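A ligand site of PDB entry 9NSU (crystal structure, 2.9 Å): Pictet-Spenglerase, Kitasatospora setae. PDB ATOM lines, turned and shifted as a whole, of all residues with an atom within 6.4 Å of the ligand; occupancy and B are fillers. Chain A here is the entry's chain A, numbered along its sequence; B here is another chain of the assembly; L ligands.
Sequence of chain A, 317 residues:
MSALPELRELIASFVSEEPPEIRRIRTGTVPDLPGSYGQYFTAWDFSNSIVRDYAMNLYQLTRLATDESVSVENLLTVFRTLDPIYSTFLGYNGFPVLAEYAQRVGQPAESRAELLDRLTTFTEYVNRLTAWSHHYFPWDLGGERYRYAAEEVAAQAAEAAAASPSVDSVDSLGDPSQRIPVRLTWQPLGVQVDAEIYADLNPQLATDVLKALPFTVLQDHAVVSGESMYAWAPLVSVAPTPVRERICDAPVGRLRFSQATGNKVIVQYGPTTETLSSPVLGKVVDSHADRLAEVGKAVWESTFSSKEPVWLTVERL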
ATOM      1  N   ARG A  52       2.927  27.443   9.945  1.00  0.00           N
ATOM      2  CA  ARG A  52       3.235  28.225   8.725  1.00  0.00           C
ATOM      3  C   ARG A  52       2.122  28.047   7.691  1.00  0.00           C
ATOM      4  O   ARG A  52       1.590  29.068   7.186  1.00  0.00           O
ATOM      5  CB  ARG A  52       4.549  27.736   8.105  1.00  0.00           C
ATOM      6  CG  ARG A  52       4.762  28.393   6.756  1.00  0.00           C
ATOM      7  CD  ARG A  52       5.159  27.415   5.669  1.00  0.00           C
ATOM      8  NE  ARG A  52       6.359  26.660   6.032  1.00  0.00           N
ATOM      9  CZ  ARG A  52       6.408  25.335   6.145  1.00  0.00           C
ATOM     10  NH1 ARG A  52       5.332  24.614   5.920  1.00  0.00           N
ATOM     11  NH2 ARG A  52       7.542  24.749   6.479  1.00  0.00           N
ATOM     12  N   ASP A  53       1.782  26.802   7.378  1.00  0.00           N
ATOM     13  CA  ASP A  53       0.794  26.546   6.290  1.00  0.00           C
ATOM     14  C   ASP A  53      -0.594  26.927   6.769  1.00  0.00           C
ATOM     15  O   ASP A  53      -1.389  27.468   5.973  1.00  0.00           O
ATOM     16  CB  ASP A  53       0.864  25.098   5.840  1.00  0.00           C
ATOM     17  CG  ASP A  53       2.272  24.603   5.529  1.00  0.00           C
ATOM     18  OD1 ASP A  53       2.819  24.965   4.466  1.00  0.00           O
ATOM     19  OD2 ASP A  53       2.823  23.832   6.341  1.00  0.00           O
ATOM     20  N   MET A  56      -0.716  30.579   6.021  1.00  0.00           N
ATOM     21  CA  MET A  56      -0.934  30.929   4.592  1.00  0.00           C
ATOM     22  C   MET A  56      -2.402  30.690   4.255  1.00  0.00           C
ATOM     23  O   MET A  56      -3.004  31.492   3.523  1.00  0.00           O
ATOM     24  CB  MET A  56      -0.030  30.063   3.725  1.00  0.00           C
ATOM     25  CG  MET A  56       1.229  29.768   4.459  1.00  0.00           C
ATOM     26  SD  MET A  56       2.441  28.964   3.417  1.00  0.00           S
ATOM     27  CE  MET A  56       2.312  30.050   1.986  1.00  0.00           C
ATOM     28  N   HIS A 134       9.980  30.171  12.711  1.00  0.00           N
ATOM     29  CA  HIS A 134      10.922  30.208  11.565  1.00  0.00           C
ATOM     30  C   HIS A 134      12.305  30.604  12.095  1.00  0.00           C
ATOM     31  O   HIS A 134      13.313  30.001  11.712  1.00  0.00           O
ATOM     32  CB  HIS A 134      10.418  31.209  10.519  1.00  0.00           C
ATOM     33  CG  HIS A 134      11.274  31.311   9.307  1.00  0.00           C
ATOM     34  ND1 HIS A 134      12.656  31.326   9.350  1.00  0.00           N
ATOM     35  CD2 HIS A 134      10.949  31.443   8.008  1.00  0.00           C
ATOM     36  CE1 HIS A 134      13.137  31.440   8.116  1.00  0.00           C
ATOM     37  NE2 HIS A 134      12.115  31.525   7.282  1.00  0.00           N
ATOM     38  N   HIS A 221      16.485  34.845   7.391  1.00  0.00           N
ATOM     39  CA  HIS A 221      16.898  34.514   6.018  1.00  0.00           C
ATOM     40  C   HIS A 221      15.984  33.443   5.439  1.00  0.00           C
ATOM     41  O   HIS A 221      15.521  32.538   6.184  1.00  0.00           O
ATOM     42  CB  HIS A 221      18.333  33.994   6.062  1.00  0.00           C
ATOM     43  CG  HIS A 221      19.093  34.139   4.798  1.00  0.00           C
ATOM     44  ND1 HIS A 221      18.569  33.806   3.568  1.00  0.00           N
ATOM     45  CD2 HIS A 221      20.341  34.564   4.577  1.00  0.00           C
ATOM     46  CE1 HIS A 221      19.482  34.036   2.645  1.00  0.00           C
ATOM     47  NE2 HIS A 221      20.566  34.490   3.231  1.00  0.00           N
ATOM     48  N   ALA A 222      15.698  33.568   4.147  1.00  0.00           N
ATOM     49  CA  ALA A 222      14.982  32.491   3.429  1.00  0.00           C
ATOM     50  C   ALA A 222      15.819  31.225   3.484  1.00  0.00           C
ATOM     51  O   ALA A 222      17.053  31.274   3.307  1.00  0.00           O
ATOM     52  CB  ALA A 222      14.750  32.935   2.007  1.00  0.00           C
ATOM     53  N   VAL A 223      15.158  30.078   3.690  1.00  0.00           N
ATOM     54  CA  VAL A 223      15.940  28.818   3.872  1.00  0.00           C
ATOM     55  C   VAL A 223      15.946  27.933   2.622  1.00  0.00           C
ATOM     56  O   VAL A 223      16.693  26.946   2.604  1.00  0.00           O
ATOM     57  CB  VAL A 223      15.378  28.058   5.097  1.00  0.00           C
ATOM     58  CG1 VAL A 223      15.907  28.649   6.393  1.00  0.00           C
ATOM     59  CG2 VAL A 223      13.855  28.084   5.108  1.00  0.00           C
ATOM     60  N   VAL A 224      15.174  28.266   1.588  1.00  0.00           N
ATOM     61  CA  VAL A 224      15.238  27.442   0.352  1.00  0.00           C
ATOM     62  C   VAL A 224      15.559  28.335  -0.842  1.00  0.00           C
ATOM     63  O   VAL A 224      16.356  27.910  -1.698  1.00  0.00           O
ATOM     64  CB  VAL A 224      13.900  26.676   0.148  1.00  0.00           C
ATOM     65  CG1 VAL A 224      13.408  26.045   1.446  1.00  0.00           C
ATOM     66  CG2 VAL A 224      12.783  27.540  -0.435  1.00  0.00           C
ATOM     67  N   SER A 225      15.045  29.573  -0.859  1.00  0.00           N
ATOM     68  CA  SER A 225      15.135  30.438  -2.063  1.00  0.00           C
ATOM     69  C   SER A 225      16.594  30.697  -2.464  1.00  0.00           C
ATOM     70  O   SER A 225      16.880  30.694  -3.678  1.00  0.00           O
ATOM     71  CB  SER A 225      14.439  31.764  -1.869  1.00  0.00           C
ATOM     72  OG  SER A 225      13.371  31.683  -0.935  1.00  0.00           O
ATOM     73  N   GLY A 226      17.454  30.982  -1.490  1.00  0.00           N
ATOM     74  CA  GLY A 226      18.844  31.327  -1.823  1.00  0.00           C
ATOM     75  C   GLY A 226      19.326  32.573  -1.096  1.00  0.00           C
ATOM     76  O   GLY A 226      19.233  32.601   0.152  1.00  0.00           O
ATOM     77  N   TYR A 230      14.097  38.056   4.696  1.00  0.00           N
ATOM     78  CA  TYR A 230      12.720  38.603   4.826  1.00  0.00           C
ATOM     79  C   TYR A 230      12.421  38.845   6.307  1.00  0.00           C
ATOM     80  O   TYR A 230      13.126  38.294   7.187  1.00  0.00           O
ATOM     81  CB  TYR A 230      11.645  37.721   4.160  1.00  0.00           C
ATOM     82  CG  TYR A 230      11.729  36.206   4.303  1.00  0.00           C
ATOM     83  CD1 TYR A 230      11.641  35.584   5.549  1.00  0.00           C
ATOM     84  CD2 TYR A 230      11.847  35.382   3.182  1.00  0.00           C
ATOM     85  CE1 TYR A 230      11.709  34.203   5.675  1.00  0.00           C
ATOM     86  CE2 TYR A 230      11.904  33.998   3.295  1.00  0.00           C
ATOM     87  CZ  TYR A 230      11.841  33.411   4.543  1.00  0.00           C
ATOM     88  OH  TYR A 230      11.895  32.058   4.704  1.00  0.00           O
ATOM     89  N   ILE A 247      11.378  36.709  -9.855  1.00  0.00           N
ATOM     90  CA  ILE A 247      12.544  37.064  -9.003  1.00  0.00           C
ATOM     91  C   ILE A 247      13.885  36.846  -9.706  1.00  0.00           C
ATOM     92  O   ILE A 247      14.845  37.500  -9.289  1.00  0.00           O
ATOM     93  CB  ILE A 247      12.432  36.277  -7.692  1.00  0.00           C
ATOM     94  CG1 ILE A 247      13.038  34.906  -7.841  1.00  0.00           C
ATOM     95  CG2 ILE A 247      10.967  36.179  -7.300  1.00  0.00           C
ATOM     96  CD1 ILE A 247      12.916  34.083  -6.582  1.00  0.00           C
ATOM     97  N   SER A 258       5.369  39.909   0.326  1.00  0.00           N
ATOM     98  CA  SER A 258       4.563  38.702   0.021  1.00  0.00           C
ATOM     99  C   SER A 258       3.420  38.601   1.050  1.00  0.00           C
ATOM    100  O   SER A 258       3.656  38.170   2.194  1.00  0.00           O
ATOM    101  CB  SER A 258       5.413  37.474   0.004  1.00  0.00           C
ATOM    102  OG  SER A 258       4.601  36.338  -0.267  1.00  0.00           O
ATOM    103  N   THR A 261       3.162  34.368   1.785  1.00  0.00           N
ATOM    104  CA  THR A 261       4.015  33.490   2.625  1.00  0.00           C
ATOM    105  C   THR A 261       4.194  34.057   4.022  1.00  0.00           C
ATOM    106  O   THR A 261       4.866  33.413   4.844  1.00  0.00           O
ATOM    107  CB  THR A 261       5.337  33.231   1.930  1.00  0.00           C
ATOM    108  OG1 THR A 261       6.140  32.479   2.828  1.00  0.00           O
ATOM    109  CG2 THR A 261       6.018  34.542   1.596  1.00  0.00           C
ATOM    110  N   LYS A 264       5.290  39.184   4.574  1.00  0.00           N
ATOM    111  CA  LYS A 264       6.737  39.425   4.709  1.00  0.00           C
ATOM    112  C   LYS A 264       7.237  40.528   3.805  1.00  0.00           C
ATOM    113  O   LYS A 264       6.575  40.843   2.800  1.00  0.00           O
ATOM    114  CB  LYS A 264       7.459  38.093   4.457  1.00  0.00           C
ATOM    115  CG  LYS A 264       7.342  37.135   5.636  1.00  0.00           C
ATOM    116  CD  LYS A 264       8.411  36.065   5.541  1.00  0.00           C
ATOM    117  CE  LYS A 264       8.271  35.338   4.253  1.00  0.00           C
ATOM    118  NZ  LYS A 264       7.472  34.119   4.437  1.00  0.00           N
ATOM    119  N   GLY B  35      17.066  24.921  -1.993  1.00  0.00           N
ATOM    120  CA  GLY B  35      17.810  25.011  -0.730  1.00  0.00           C
ATOM    121  C   GLY B  35      18.768  26.189  -0.723  1.00  0.00           C
ATOM    122  O   GLY B  35      19.095  26.722  -1.805  1.00  0.00           O
ATOM    123  N   SER B  36      19.221  26.575   0.461  1.00  0.00           N
ATOM    124  CA  SER B  36      20.115  27.740   0.598  1.00  0.00           C
ATOM    125  C   SER B  36      21.541  27.281   0.862  1.00  0.00           C
ATOM    126  O   SER B  36      21.746  26.402   1.716  1.00  0.00           O
ATOM    127  CB  SER B  36      19.647  28.637   1.716  1.00  0.00           C
ATOM    128  OG  SER B  36      18.811  29.667   1.214  1.00  0.00           O
ATOM    129  N   PHE B  46      10.730  21.566   3.693  1.00  0.00           N
ATOM    130  CA  PHE B  46       9.625  22.352   3.096  1.00  0.00           C
ATOM    131  C   PHE B  46       8.764  21.458   2.221  1.00  0.00           C
ATOM    132  O   PHE B  46       7.547  21.441   2.378  1.00  0.00           O
ATOM    133  CB  PHE B  46      10.213  23.510   2.304  1.00  0.00           C
ATOM    134  CG  PHE B  46      10.211  24.777   3.126  1.00  0.00           C
ATOM    135  CD1 PHE B  46      11.053  24.901   4.218  1.00  0.00           C
ATOM    136  CD2 PHE B  46       9.327  25.798   2.831  1.00  0.00           C
ATOM    137  CE1 PHE B  46      11.037  26.045   4.980  1.00  0.00           C
ATOM    138  CE2 PHE B  46       9.309  26.941   3.602  1.00  0.00           C
ATOM    139  CZ  PHE B  46      10.167  27.066   4.667  1.00  0.00           C
ATOM    140  N   ILE B  50       4.895  20.822   3.044  1.00  0.00           N
ATOM    141  CA  ILE B  50       3.919  21.506   2.159  1.00  0.00           C
ATOM    142  C   ILE B  50       3.079  20.446   1.441  1.00  0.00           C
ATOM    143  O   ILE B  50       1.880  20.660   1.244  1.00  0.00           O
ATOM    144  CB  ILE B  50       4.616  22.435   1.164  1.00  0.00           C
ATOM    145  CG1 ILE B  50       5.594  23.398   1.837  1.00  0.00           C
ATOM    146  CG2 ILE B  50       3.573  23.217   0.380  1.00  0.00           C
ATOM    147  CD1 ILE B  50       4.974  24.710   2.283  1.00  0.00           C
ATOM    148  N   ILE B  85      -0.834  28.972  -4.121  1.00  0.00           N
ATOM    149  CA  ILE B  85       0.308  29.257  -3.225  1.00  0.00           C
ATOM    150  C   ILE B  85       0.999  27.920  -2.922  1.00  0.00           C
ATOM    151  O   ILE B  85       2.241  27.856  -2.914  1.00  0.00           O
ATOM    152  CB  ILE B  85      -0.155  29.981  -1.945  1.00  0.00           C
ATOM    153  CG1 ILE B  85       1.010  30.692  -1.277  1.00  0.00           C
ATOM    154  CG2 ILE B  85      -0.837  29.031  -0.972  1.00  0.00           C
ATOM    155  CD1 ILE B  85       1.654  31.759  -2.139  1.00  0.00           C
ATOM    156  N   TYR B  86       0.217  26.865  -2.752  1.00  0.00           N
ATOM    157  CA  TYR B  86       0.789  25.515  -2.507  1.00  0.00           C
ATOM    158  C   TYR B  86       1.204  24.875  -3.821  1.00  0.00           C
ATOM    159  O   TYR B  86       2.326  24.331  -3.918  1.00  0.00           O
ATOM    160  CB  TYR B  86      -0.288  24.665  -1.832  1.00  0.00           C
ATOM    161  CG  TYR B  86      -0.570  24.988  -0.382  1.00  0.00           C
ATOM    162  CD1 TYR B  86       0.215  24.478   0.626  1.00  0.00           C
ATOM    163  CD2 TYR B  86      -1.644  25.784  -0.034  1.00  0.00           C
ATOM    164  CE1 TYR B  86      -0.043  24.749   1.956  1.00  0.00           C
ATOM    165  CE2 TYR B  86      -1.912  26.084   1.289  1.00  0.00           C
ATOM    166  CZ  TYR B  86      -1.110  25.558   2.288  1.00  0.00           C
ATOM    167  OH  TYR B  86      -1.373  25.838   3.597  1.00  0.00           O
ATOM    168  N   PHE B  89       4.395  26.545  -5.760  1.00  0.00           N
ATOM    169  CA  PHE B  89       5.601  26.383  -4.915  1.00  0.00           C
ATOM    170  C   PHE B  89       6.077  24.932  -4.992  1.00  0.00           C
ATOM    171  O   PHE B  89       7.224  24.675  -5.378  1.00  0.00           O
ATOM    172  CB  PHE B  89       5.274  26.774  -3.480  1.00  0.00           C
ATOM    173  CG  PHE B  89       6.356  26.392  -2.478  1.00  0.00           C
ATOM    174  CD1 PHE B  89       7.470  27.190  -2.302  1.00  0.00           C
ATOM    175  CD2 PHE B  89       6.243  25.234  -1.726  1.00  0.00           C
ATOM    176  CE1 PHE B  89       8.446  26.843  -1.387  1.00  0.00           C
ATOM    177  CE2 PHE B  89       7.219  24.887  -0.811  1.00  0.00           C
ATOM    178  CZ  PHE B  89       8.326  25.691  -0.645  1.00  0.00           C
ATOM    179  N   TYR B  92       7.821  24.109  -7.952  1.00  0.00           N
ATOM    180  CA  TYR B  92       9.252  24.486  -8.031  1.00  0.00           C
ATOM    181  C   TYR B  92      10.109  23.502  -7.254  1.00  0.00           C
ATOM    182  O   TYR B  92      11.221  23.194  -7.721  1.00  0.00           O
ATOM    183  CB  TYR B  92       9.449  25.922  -7.560  1.00  0.00           C
ATOM    184  CG  TYR B  92       9.066  26.882  -8.673  1.00  0.00           C
ATOM    185  CD1 TYR B  92       9.966  27.245  -9.654  1.00  0.00           C
ATOM    186  CD2 TYR B  92       7.771  27.388  -8.744  1.00  0.00           C
ATOM    187  CE1 TYR B  92       9.602  28.116 -10.679  1.00  0.00           C
ATOM    188  CE2 TYR B  92       7.401  28.248  -9.761  1.00  0.00           C
ATOM    189  CZ  TYR B  92       8.311  28.614 -10.729  1.00  0.00           C
ATOM    190  OH  TYR B  92       7.935  29.468 -11.717  1.00  0.00           O
ATOM    191  N   ASN B  93       9.631  23.014  -6.121  1.00  0.00           N
ATOM    192  CA  ASN B  93      10.523  22.141  -5.314  1.00  0.00           C
ATOM    193  C   ASN B  93       9.948  20.735  -5.219  1.00  0.00           C
ATOM    194  O   ASN B  93       9.270  20.439  -4.199  1.00  0.00           O
ATOM    195  CB  ASN B  93      10.770  22.732  -3.939  1.00  0.00           C
ATOM    196  CG  ASN B  93      10.701  24.229  -3.999  1.00  0.00           C
ATOM    197  OD1 ASN B  93      11.388  24.851  -4.812  1.00  0.00           O
ATOM    198  ND2 ASN B  93       9.838  24.818  -3.194  1.00  0.00           N
HETATM  199  C1  LIG L   1      10.065  31.543  -0.705  1.00  0.00           C
HETATM  200  C2  LIG L   1      10.383  31.310  -2.129  1.00  0.00           C
HETATM  201  C3  LIG L   1      10.360  29.811  -2.432  1.00  0.00           C
HETATM  202  C4  LIG L   1      11.368  29.393  -3.484  1.00  0.00           C
HETATM  203  C5  LIG L   1      10.911  30.633   1.471  1.00  0.00           C
HETATM  204  C6  LIG L   1       9.780  29.628   1.529  1.00  0.00           C
HETATM  205  C7  LIG L   1       8.638  29.915   0.588  1.00  0.00           C
HETATM  206  C8  LIG L   1       8.761  30.801  -0.428  1.00  0.00           C
HETATM  207  C9  LIG L   1       6.719  30.066  -0.580  1.00  0.00           C
HETATM  208  C10 LIG L   1       5.393  29.797  -0.936  1.00  0.00           C
HETATM  209  C11 LIG L   1       4.646  28.889  -0.207  1.00  0.00           C
HETATM  210  C12 LIG L   1       5.228  28.258   0.881  1.00  0.00           C
HETATM  211  C13 LIG L   1       6.548  28.516   1.244  1.00  0.00           C
HETATM  212  C14 LIG L   1       7.303  29.438   0.498  1.00  0.00           C
HETATM  213  C15 LIG L   1      12.260  30.149   2.037  1.00  0.00           C
HETATM  214  N1  LIG L   1      11.225  30.952   0.070  1.00  0.00           N
HETATM  215  N2  LIG L   1       7.610  30.874  -1.124  1.00  0.00           N
HETATM  216  O1  LIG L   1      11.385  29.931  -4.617  1.00  0.00           O
HETATM  217  O2  LIG L   1      12.180  28.483  -3.202  1.00  0.00           O
HETATM  218  O3  LIG L   1      13.240  30.064   1.257  1.00  0.00           O
HETATM  219  O4  LIG L   1      12.423  29.873   3.251  1.00  0.00           O
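The backbone NH (N) of Ser 225 sits at hydrogen-bond distance from an oxygen (O3) of the ligand, 2.8 Å away.
The side-chain hydroxyl of Ser 225 is in hydrogen-bond range of a nitrogen (N1) of the ligand (2.5 Å).
An oxygen (O3) of the ligand lies within hydrogen-bond range of the backbone NH (N) of Val 224.
The side-chain hydroxyl (OH) of Tyr 230 is in hydrogen-bond range of an oxygen (O4) of the ligand.
An oxygen (O4) of the ligand is in hydrogen-bond range of the backbone NH of Val 223, at 2.8 Å.
The backbone carbonyl oxygen (O) of Val 224 lies within hydrogen-bond range of the backbone NH (N) of Gly 35 of chain B, 3.1 Å away.
The side-chain hydroxyl (OH) of Tyr 230 lies within hydrogen-bond range of a ring nitrogen (NE2) of His 134 (2.6 Å).
N of Ser 36 of chain B is in hydrogen-bond range of O of Val 223.
O of Ala 222 is in hydrogen-bond range of OG of Ser 36 of chain B (3.2 Å).
The backbone carbonyl oxygen (O) of Phe 89 of chain B lies close to the side-chain amide nitrogen (ND2) of Asn 93 of chain B.
CE of Met 56 touches C11 of the ligand (3.4 Å).
CB of Ala 222 touches O3 of the ligand (3.3 Å).
Phe 46 of chain B touches the ligand (CE2 to C6, 3.4 Å).
CD1 of Ile 50 of chain B touches C12 of the ligand, at 3.8 Å.
Ile 85 of chain B touches the ligand.
CE1 of Phe 89 of chain B touches C14 of the ligand, at 3.4 Å.
Hydrophobic or aromatic side chains within 4 Å of the ligand: Met 56, Ala 222, Val 223, Val 224, Tyr 230, Phe 46 of chain B, Ile 50 of chain B and Phe 89 of chain B.
Of the 24 residues printed, 10 come within 4 Å of the ligand.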
